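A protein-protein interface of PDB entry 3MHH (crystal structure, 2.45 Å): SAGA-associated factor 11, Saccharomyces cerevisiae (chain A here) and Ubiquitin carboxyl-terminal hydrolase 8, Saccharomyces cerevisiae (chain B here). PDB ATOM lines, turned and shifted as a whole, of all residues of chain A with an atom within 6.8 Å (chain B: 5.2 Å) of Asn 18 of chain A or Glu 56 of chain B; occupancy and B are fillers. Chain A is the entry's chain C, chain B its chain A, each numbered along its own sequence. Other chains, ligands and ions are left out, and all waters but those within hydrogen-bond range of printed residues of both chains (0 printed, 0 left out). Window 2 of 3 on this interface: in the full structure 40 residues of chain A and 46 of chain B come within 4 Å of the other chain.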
ATOM      1  N   ASN A  13     -11.888 -15.485  11.553  1.00  0.00           N
ATOM      2  CA  ASN A  13     -12.011 -16.287  10.343  1.00  0.00           C
ATOM      3  C   ASN A  13     -10.675 -16.975  10.064  1.00  0.00           C
ATOM      4  O   ASN A  13     -10.630 -18.157   9.726  1.00  0.00           O
ATOM      5  CB  ASN A  13     -12.456 -15.437   9.154  1.00  0.00           C
ATOM      6  CG  ASN A  13     -13.945 -15.113   9.190  1.00  0.00           C
ATOM      7  OD1 ASN A  13     -14.790 -15.988   8.984  1.00  0.00           O
ATOM      8  ND2 ASN A  13     -14.275 -13.847   9.439  1.00  0.00           N
ATOM      9  N   GLY A  14      -9.585 -16.245  10.266  1.00  0.00           N
ATOM     10  CA  GLY A  14      -8.252 -16.803  10.062  1.00  0.00           C
ATOM     11  C   GLY A  14      -7.985 -17.993  10.965  1.00  0.00           C
ATOM     12  O   GLY A  14      -7.402 -18.991  10.535  1.00  0.00           O
ATOM     13  N   ILE A  15      -8.402 -17.884  12.224  1.00  0.00           N
ATOM     14  CA  ILE A  15      -8.244 -18.985  13.175  1.00  0.00           C
ATOM     15  C   ILE A  15      -9.108 -20.174  12.756  1.00  0.00           C
ATOM     16  O   ILE A  15      -8.636 -21.297  12.735  1.00  0.00           O
ATOM     17  CB  ILE A  15      -8.586 -18.546  14.604  1.00  0.00           C
ATOM     18  CG1 ILE A  15      -7.546 -17.545  15.096  1.00  0.00           C
ATOM     19  CG2 ILE A  15      -8.663 -19.739  15.560  1.00  0.00           C
ATOM     20  CD1 ILE A  15      -7.910 -16.921  16.418  1.00  0.00           C
ATOM     21  N   LEU A  16     -10.351 -19.919  12.374  1.00  0.00           N
ATOM     22  CA  LEU A  16     -11.238 -20.982  11.951  1.00  0.00           C
ATOM     23  C   LEU A  16     -10.702 -21.684  10.715  1.00  0.00           C
ATOM     24  O   LEU A  16     -10.801 -22.908  10.601  1.00  0.00           O
ATOM     25  CB  LEU A  16     -12.650 -20.445  11.672  1.00  0.00           C
ATOM     26  CG  LEU A  16     -13.643 -21.527  11.221  1.00  0.00           C
ATOM     27  CD1 LEU A  16     -13.861 -22.509  12.341  1.00  0.00           C
ATOM     28  CD2 LEU A  16     -14.984 -20.943  10.731  1.00  0.00           C
ATOM     29  N   ASN A  17     -10.145 -20.902   9.792  1.00  0.00           N
ATOM     30  CA  ASN A  17      -9.624 -21.416   8.517  1.00  0.00           C
ATOM     31  C   ASN A  17      -8.412 -22.330   8.738  1.00  0.00           C
ATOM     32  O   ASN A  17      -8.305 -23.408   8.146  1.00  0.00           O
ATOM     33  CB  ASN A  17      -9.265 -20.225   7.621  1.00  0.00           C
ATOM     34  CG  ASN A  17      -8.738 -20.639   6.249  1.00  0.00           C
ATOM     35  OD1 ASN A  17      -7.551 -20.469   5.966  1.00  0.00           O
ATOM     36  ND2 ASN A  17      -9.623 -21.139   5.382  1.00  0.00           N
ATOM     37  N   ASN A  18      -7.507 -21.909   9.615  1.00  0.00           N
ATOM     38  CA  ASN A  18      -6.417 -22.777  10.046  1.00  0.00           C
ATOM     39  C   ASN A  18      -6.986 -24.098  10.581  1.00  0.00           C
ATOM     40  O   ASN A  18      -6.557 -25.186  10.171  1.00  0.00           O
ATOM     41  CB  ASN A  18      -5.566 -22.105  11.133  1.00  0.00           C
ATOM     42  CG  ASN A  18      -4.560 -21.092  10.568  1.00  0.00           C
ATOM     43  OD1 ASN A  18      -3.555 -20.775  11.207  1.00  0.00           O
ATOM     44  ND2 ASN A  18      -4.830 -20.584   9.385  1.00  0.00           N
ATOM     45  N   LEU A  19      -7.963 -24.004  11.479  1.00  0.00           N
ATOM     46  CA  LEU A  19      -8.529 -25.207  12.075  1.00  0.00           C
ATOM     47  C   LEU A  19      -9.159 -26.028  10.968  1.00  0.00           C
ATOM     48  O   LEU A  19      -8.974 -27.252  10.891  1.00  0.00           O
ATOM     49  CB  LEU A  19      -9.568 -24.865  13.144  1.00  0.00           C
ATOM     50  CG  LEU A  19      -9.058 -24.394  14.510  1.00  0.00           C
ATOM     51  CD1 LEU A  19     -10.156 -23.679  15.297  1.00  0.00           C
ATOM     52  CD2 LEU A  19      -8.482 -25.547  15.336  1.00  0.00           C
ATOM     53  N   LEU A  20      -9.887 -25.349  10.087  1.00  0.00           N
ATOM     54  CA  LEU A  20     -10.615 -26.048   9.034  1.00  0.00           C
ATOM     55  C   LEU A  20      -9.669 -26.711   8.029  1.00  0.00           C
ATOM     56  O   LEU A  20      -9.835 -27.881   7.709  1.00  0.00           O
ATOM     57  CB  LEU A  20     -11.597 -25.106   8.338  1.00  0.00           C
ATOM     58  CG  LEU A  20     -12.906 -24.841   9.084  1.00  0.00           C
ATOM     59  CD1 LEU A  20     -13.736 -23.776   8.368  1.00  0.00           C
ATOM     60  CD2 LEU A  20     -13.706 -26.125   9.237  1.00  0.00           C
ATOM     61  N   THR A  21      -8.667 -25.976   7.554  1.00  0.00           N
ATOM     62  CA  THR A  21      -7.756 -26.503   6.529  1.00  0.00           C
ATOM     63  C   THR A  21      -6.889 -27.645   7.065  1.00  0.00           C
ATOM     64  O   THR A  21      -6.646 -28.633   6.374  1.00  0.00           O
ATOM     65  CB  THR A  21      -6.874 -25.384   5.877  1.00  0.00           C
ATOM     66  OG1 THR A  21      -6.297 -24.551   6.888  1.00  0.00           O
ATOM     67  CG2 THR A  21      -7.713 -24.501   4.942  1.00  0.00           C
ATOM     68  N   THR A  22      -6.455 -27.541   8.310  1.00  0.00           N
ATOM     69  CA  THR A  22      -5.651 -28.602   8.900  1.00  0.00           C
ATOM     70  C   THR A  22      -6.453 -29.906   8.955  1.00  0.00           C
ATOM     71  O   THR A  22      -5.928 -30.984   8.674  1.00  0.00           O
ATOM     72  CB  THR A  22      -5.166 -28.241  10.327  1.00  0.00           C
ATOM     73  OG1 THR A  22      -4.413 -27.008  10.305  1.00  0.00           O
ATOM     74  CG2 THR A  22      -4.309 -29.380  10.888  1.00  0.00           C
ATOM     75  N   LEU A  23      -7.721 -29.807   9.341  1.00  0.00           N
ATOM     76  CA  LEU A  23      -8.560 -30.983   9.465  1.00  0.00           C
ATOM     77  C   LEU A  23      -8.880 -31.598   8.097  1.00  0.00           C
ATOM     78  O   LEU A  23      -8.860 -32.823   7.953  1.00  0.00           O
ATOM     79  CB  LEU A  23      -9.845 -30.639  10.201  1.00  0.00           C
ATOM     80  CG  LEU A  23     -10.826 -31.800  10.377  1.00  0.00           C
ATOM     81  CD1 LEU A  23     -10.185 -32.982  11.145  1.00  0.00           C
ATOM     82  CD2 LEU A  23     -12.086 -31.300  11.062  1.00  0.00           C
ATOM     83  N   GLN A  25      -6.950 -31.331   5.443  1.00  0.00           N
ATOM     84  CA  GLN A  25      -5.668 -31.853   4.962  1.00  0.00           C
ATOM     85  C   GLN A  25      -5.256 -33.136   5.657  1.00  0.00           C
ATOM     86  O   GLN A  25      -4.513 -33.927   5.097  1.00  0.00           O
ATOM     87  CB  GLN A  25      -4.561 -30.809   5.104  1.00  0.00           C
ATOM     88  CG  GLN A  25      -4.700 -29.673   4.123  1.00  0.00           C
ATOM     89  CD  GLN A  25      -3.922 -28.433   4.518  1.00  0.00           C
ATOM     90  OE1 GLN A  25      -2.815 -28.519   5.044  1.00  0.00           O
ATOM     91  NE2 GLN A  25      -4.476 -27.263   4.204  1.00  0.00           N
ATOM     92  N   MET B  49       2.726 -28.733  16.099  1.00  0.00           N
ATOM     93  CA  MET B  49       1.803 -28.056  15.197  1.00  0.00           C
ATOM     94  C   MET B  49       2.035 -26.566  15.192  1.00  0.00           C
ATOM     95  O   MET B  49       1.148 -25.805  14.851  1.00  0.00           O
ATOM     96  CB  MET B  49       0.357 -28.342  15.591  1.00  0.00           C
ATOM     97  CG  MET B  49      -0.072 -29.746  15.254  1.00  0.00           C
ATOM     98  SD  MET B  49      -1.551 -30.249  16.120  1.00  0.00           S
ATOM     99  CE  MET B  49      -1.633 -31.966  15.573  1.00  0.00           C
ATOM    100  N   LYS B  50       3.250 -26.168  15.551  1.00  0.00           N
ATOM    101  CA  LYS B  50       3.655 -24.774  15.549  1.00  0.00           C
ATOM    102  C   LYS B  50       4.753 -24.648  14.506  1.00  0.00           C
ATOM    103  O   LYS B  50       5.794 -25.290  14.616  1.00  0.00           O
ATOM    104  CB  LYS B  50       4.185 -24.390  16.931  1.00  0.00           C
ATOM    105  CG  LYS B  50       4.935 -23.053  17.021  1.00  0.00           C
ATOM    106  CD  LYS B  50       4.082 -21.951  17.611  1.00  0.00           C
ATOM    107  CE  LYS B  50       4.926 -20.953  18.403  1.00  0.00           C
ATOM    108  NZ  LYS B  50       5.400 -21.521  19.695  1.00  0.00           N
ATOM    109  N   CYS B  51       4.509 -23.842  13.482  1.00  0.00           N
ATOM    110  CA  CYS B  51       5.462 -23.689  12.404  1.00  0.00           C
ATOM    111  C   CYS B  51       6.646 -22.869  12.875  1.00  0.00           C
ATOM    112  O   CYS B  51       6.467 -21.804  13.440  1.00  0.00           O
ATOM    113  CB  CYS B  51       4.789 -22.995  11.222  1.00  0.00           C
ATOM    114  SG  CYS B  51       5.876 -22.565   9.836  1.00  0.00           S
ATOM    115  N   CYS B  54       6.566 -19.151  10.534  1.00  0.00           N
ATOM    116  CA  CYS B  54       5.536 -18.152  10.814  1.00  0.00           C
ATOM    117  C   CYS B  54       4.982 -18.248  12.240  1.00  0.00           C
ATOM    118  O   CYS B  54       4.221 -17.375  12.669  1.00  0.00           O
ATOM    119  CB  CYS B  54       4.406 -18.253   9.798  1.00  0.00           C
ATOM    120  SG  CYS B  54       3.493 -19.788   9.858  1.00  0.00           S
ATOM    121  N   HIS B  55       5.381 -19.290  12.970  1.00  0.00           N
ATOM    122  CA  HIS B  55       4.938 -19.503  14.346  1.00  0.00           C
ATOM    123  C   HIS B  55       3.420 -19.645  14.541  1.00  0.00           C
ATOM    124  O   HIS B  55       2.931 -19.528  15.663  1.00  0.00           O
ATOM    125  CB  HIS B  55       5.472 -18.394  15.248  1.00  0.00           C
ATOM    126  CG  HIS B  55       6.904 -18.052  14.987  1.00  0.00           C
ATOM    127  ND1 HIS B  55       7.944 -18.860  15.391  1.00  0.00           N
ATOM    128  CD2 HIS B  55       7.467 -17.010  14.328  1.00  0.00           C
ATOM    129  CE1 HIS B  55       9.088 -18.327  14.999  1.00  0.00           C
ATOM    130  NE2 HIS B  55       8.827 -17.208  14.347  1.00  0.00           N
ATOM    131  N   GLU B  56       2.678 -19.923  13.473  1.00  0.00           N
ATOM    132  CA  GLU B  56       1.243 -20.202  13.601  1.00  0.00           C
ATOM    133  C   GLU B  56       0.943 -21.645  14.019  1.00  0.00           C
ATOM    134  O   GLU B  56       1.668 -22.591  13.696  1.00  0.00           O
ATOM    135  CB  GLU B  56       0.499 -19.912  12.296  1.00  0.00           C
ATOM    136  CG  GLU B  56       0.192 -18.443  12.050  1.00  0.00           C
ATOM    137  CD  GLU B  56      -0.461 -18.207  10.701  1.00  0.00           C
ATOM    138  OE1 GLU B  56       0.114 -17.462   9.878  1.00  0.00           O
ATOM    139  OE2 GLU B  56      -1.537 -18.781  10.452  1.00  0.00           O
ATOM    140  N   ILE B  57      -0.157 -21.801  14.739  1.00  0.00           N
ATOM    141  CA  ILE B  57      -0.622 -23.101  15.102  1.00  0.00           C
ATOM    142  C   ILE B  57      -1.505 -23.547  13.962  1.00  0.00           C
ATOM    143  O   ILE B  57      -2.332 -22.773  13.484  1.00  0.00           O
ATOM    144  CB  ILE B  57      -1.455 -23.062  16.392  1.00  0.00           C
ATOM    145  CG1 ILE B  57      -0.713 -22.303  17.500  1.00  0.00           C
ATOM    146  CG2 ILE B  57      -1.800 -24.469  16.838  1.00  0.00           C
ATOM    147  CD1 ILE B  57       0.627 -22.899  17.873  1.00  0.00           C
ATOM    148  N   ASN B  58      -1.314 -24.778  13.503  1.00  0.00           N
ATOM    149  CA  ASN B  58      -2.248 -25.373  12.559  1.00  0.00           C
ATOM    150  C   ASN B  58      -2.406 -24.585  11.276  1.00  0.00           C
ATOM    151  O   ASN B  58      -3.517 -24.446  10.782  1.00  0.00           O
ATOM    152  CB  ASN B  58      -3.621 -25.473  13.217  1.00  0.00           C
ATOM    153  CG  ASN B  58      -3.715 -26.615  14.197  1.00  0.00           C
ATOM    154  OD1 ASN B  58      -4.556 -26.614  15.098  1.00  0.00           O
ATOM    155  ND2 ASN B  58      -2.861 -27.613  14.017  1.00  0.00           N
ATOM    156  N   SER B  59      -1.318 -24.036  10.745  1.00  0.00           N
ATOM    157  CA  SER B  59      -1.398 -23.315   9.478  1.00  0.00           C
ATOM    158  C   SER B  59      -1.446 -24.353   8.364  1.00  0.00           C
ATOM    159  O   SER B  59      -0.524 -24.460   7.571  1.00  0.00           O
ATOM    160  CB  SER B  59      -0.199 -22.368   9.302  1.00  0.00           C
ATOM    161  OG  SER B  59      -0.183 -21.791   8.009  1.00  0.00           O
ATOM    162  N   GLY B  60      -2.547 -25.101   8.313  1.00  0.00           N
ATOM    163  CA  GLY B  60      -2.614 -26.367   7.574  1.00  0.00           C
ATOM    164  C   GLY B  60      -1.848 -27.430   8.343  1.00  0.00           C
ATOM    165  O   GLY B  60      -1.444 -27.204   9.481  1.00  0.00           O
ATOM    166  N   ASN B  75       0.233 -24.352   4.711  1.00  0.00           N
ATOM    167  CA  ASN B  75      -0.520 -23.254   4.117  1.00  0.00           C
ATOM    168  C   ASN B  75       0.330 -22.092   3.617  1.00  0.00           C
ATOM    169  O   ASN B  75      -0.035 -21.435   2.643  1.00  0.00           O
ATOM    170  CB  ASN B  75      -1.573 -22.740   5.092  1.00  0.00           C
ATOM    171  CG  ASN B  75      -2.793 -23.604   5.124  1.00  0.00           C
ATOM    172  OD1 ASN B  75      -3.826 -23.202   5.643  1.00  0.00           O
ATOM    173  ND2 ASN B  75      -2.685 -24.809   4.574  1.00  0.00           N
ATOM    174  N   HIS B  76       1.445 -21.829   4.289  1.00  0.00           N
ATOM    175  CA  HIS B  76       2.354 -20.773   3.855  1.00  0.00           C
ATOM    176  C   HIS B  76       3.594 -21.371   3.196  1.00  0.00           C
ATOM    177  O   HIS B  76       4.584 -20.676   2.995  1.00  0.00           O
ATOM    178  CB  HIS B  76       2.768 -19.884   5.033  1.00  0.00           C
ATOM    179  CG  HIS B  76       1.638 -19.138   5.673  1.00  0.00           C
ATOM    180  ND1 HIS B  76       0.690 -18.449   4.949  1.00  0.00           N
ATOM    181  CD2 HIS B  76       1.336 -18.934   6.977  1.00  0.00           C
ATOM    182  CE1 HIS B  76      -0.160 -17.872   5.780  1.00  0.00           C
ATOM    183  NE2 HIS B  76       0.212 -18.146   7.017  1.00  0.00           N
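The side-chain carboxylate (OE2) of Glu 56 of chain B sits close to the side-chain amide oxygen (OD1) of Asn 18 of chain A, 2.9 Å away. O of Ile 57 of chain B lies close to OD1 of Asn 18 of chain A, 3.3 Å away. The backbone carbonyl oxygen (O) of Asn 58 of chain B sits at hydrogen-bond distance from the side-chain hydroxyl (OG1) of Thr 22 of chain A. OG1 of Thr 22 of chain A is in hydrogen-bond range of O of Gly 60 of chain B (3.1 Å). OG1 of Thr 21 of chain A lies within hydrogen-bond range of OD1 of Asn 75 of chain B (3.1 Å). The side-chain amide nitrogen of Gln 25 of chain A lies close to the side-chain amide nitrogen of Asn 75 of chain B (3.1 Å). The backbone carbonyl oxygen (O) of Asn 18 of chain A lies close to the backbone carbonyl oxygen (O) of Asn 58 of chain B, at 3.2 Å.
The backbone NH (N) of Cys 51 of chain B sits at hydrogen-bond distance from the backbone carbonyl oxygen (O) of Glu 56 of chain B, 3.1 Å away. SG of Cys 54 of chain B lies close to N of Glu 56 of chain B, 3.7 Å away. The side-chain carboxylate of Glu 56 of chain B lies within hydrogen-bond range of a ring nitrogen (NE2) of His 76 of chain B (2.9 Å). O of Ser 59 of chain B sits at hydrogen-bond distance from N of Asn 75 of chain B. O of Asn 18 of chain A sits at hydrogen-bond distance from OG1 of Thr 21 of chain A, at 3.4 Å. The backbone carbonyl oxygen (O) of Thr 21 of chain A lies close to the side-chain amide nitrogen (NE2) of Gln 25 of chain A (3.4 Å).
Among the printed residues, pairs that only touch across the chains: Gln 25 of chain A with Gly 60 of chain B and Asn 18 of chain A with Ser 59 of chain B.
Asn 17 of chain A touches none of the printed residues of chain B. Asn 18 of chain A touches just these residues of chain B: Glu 56 (2.9 Å), Ile 57 (3.3 Å), Asn 58 (3.1 Å) and Ser 59 (3.8 Å). Of the printed residues of chain B, Gln 25 of chain A touches Gly 60 (3.3 Å) and Asn 75 (3.1 Å). Glu 56 of chain B touches just one residue of chain A: Asn 18 (2.9 Å). Printed residues of chain A within 4 Å of Ser 59 of chain B: Asn 18 (3.8 Å). Of the printed residues of chain A, Asn 75 of chain B touches Thr 21 (3.1 Å) and Gln 25 (3.1 Å). The nearest printed residue of chain B that does not touch Thr 21 of chain A is Gly 60 of chain B (4.05 Å).
Along chain B the printed residues that touch a printed residue of chain A span positions 56 to 75. Along chain A the printed residues that touch a printed residue of chain B span positions 18 to 25. Among the printed residues, no Asp or Glu carboxylate lies within 4 Å of a Lys or Arg side-chain nitrogen of the other chain.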
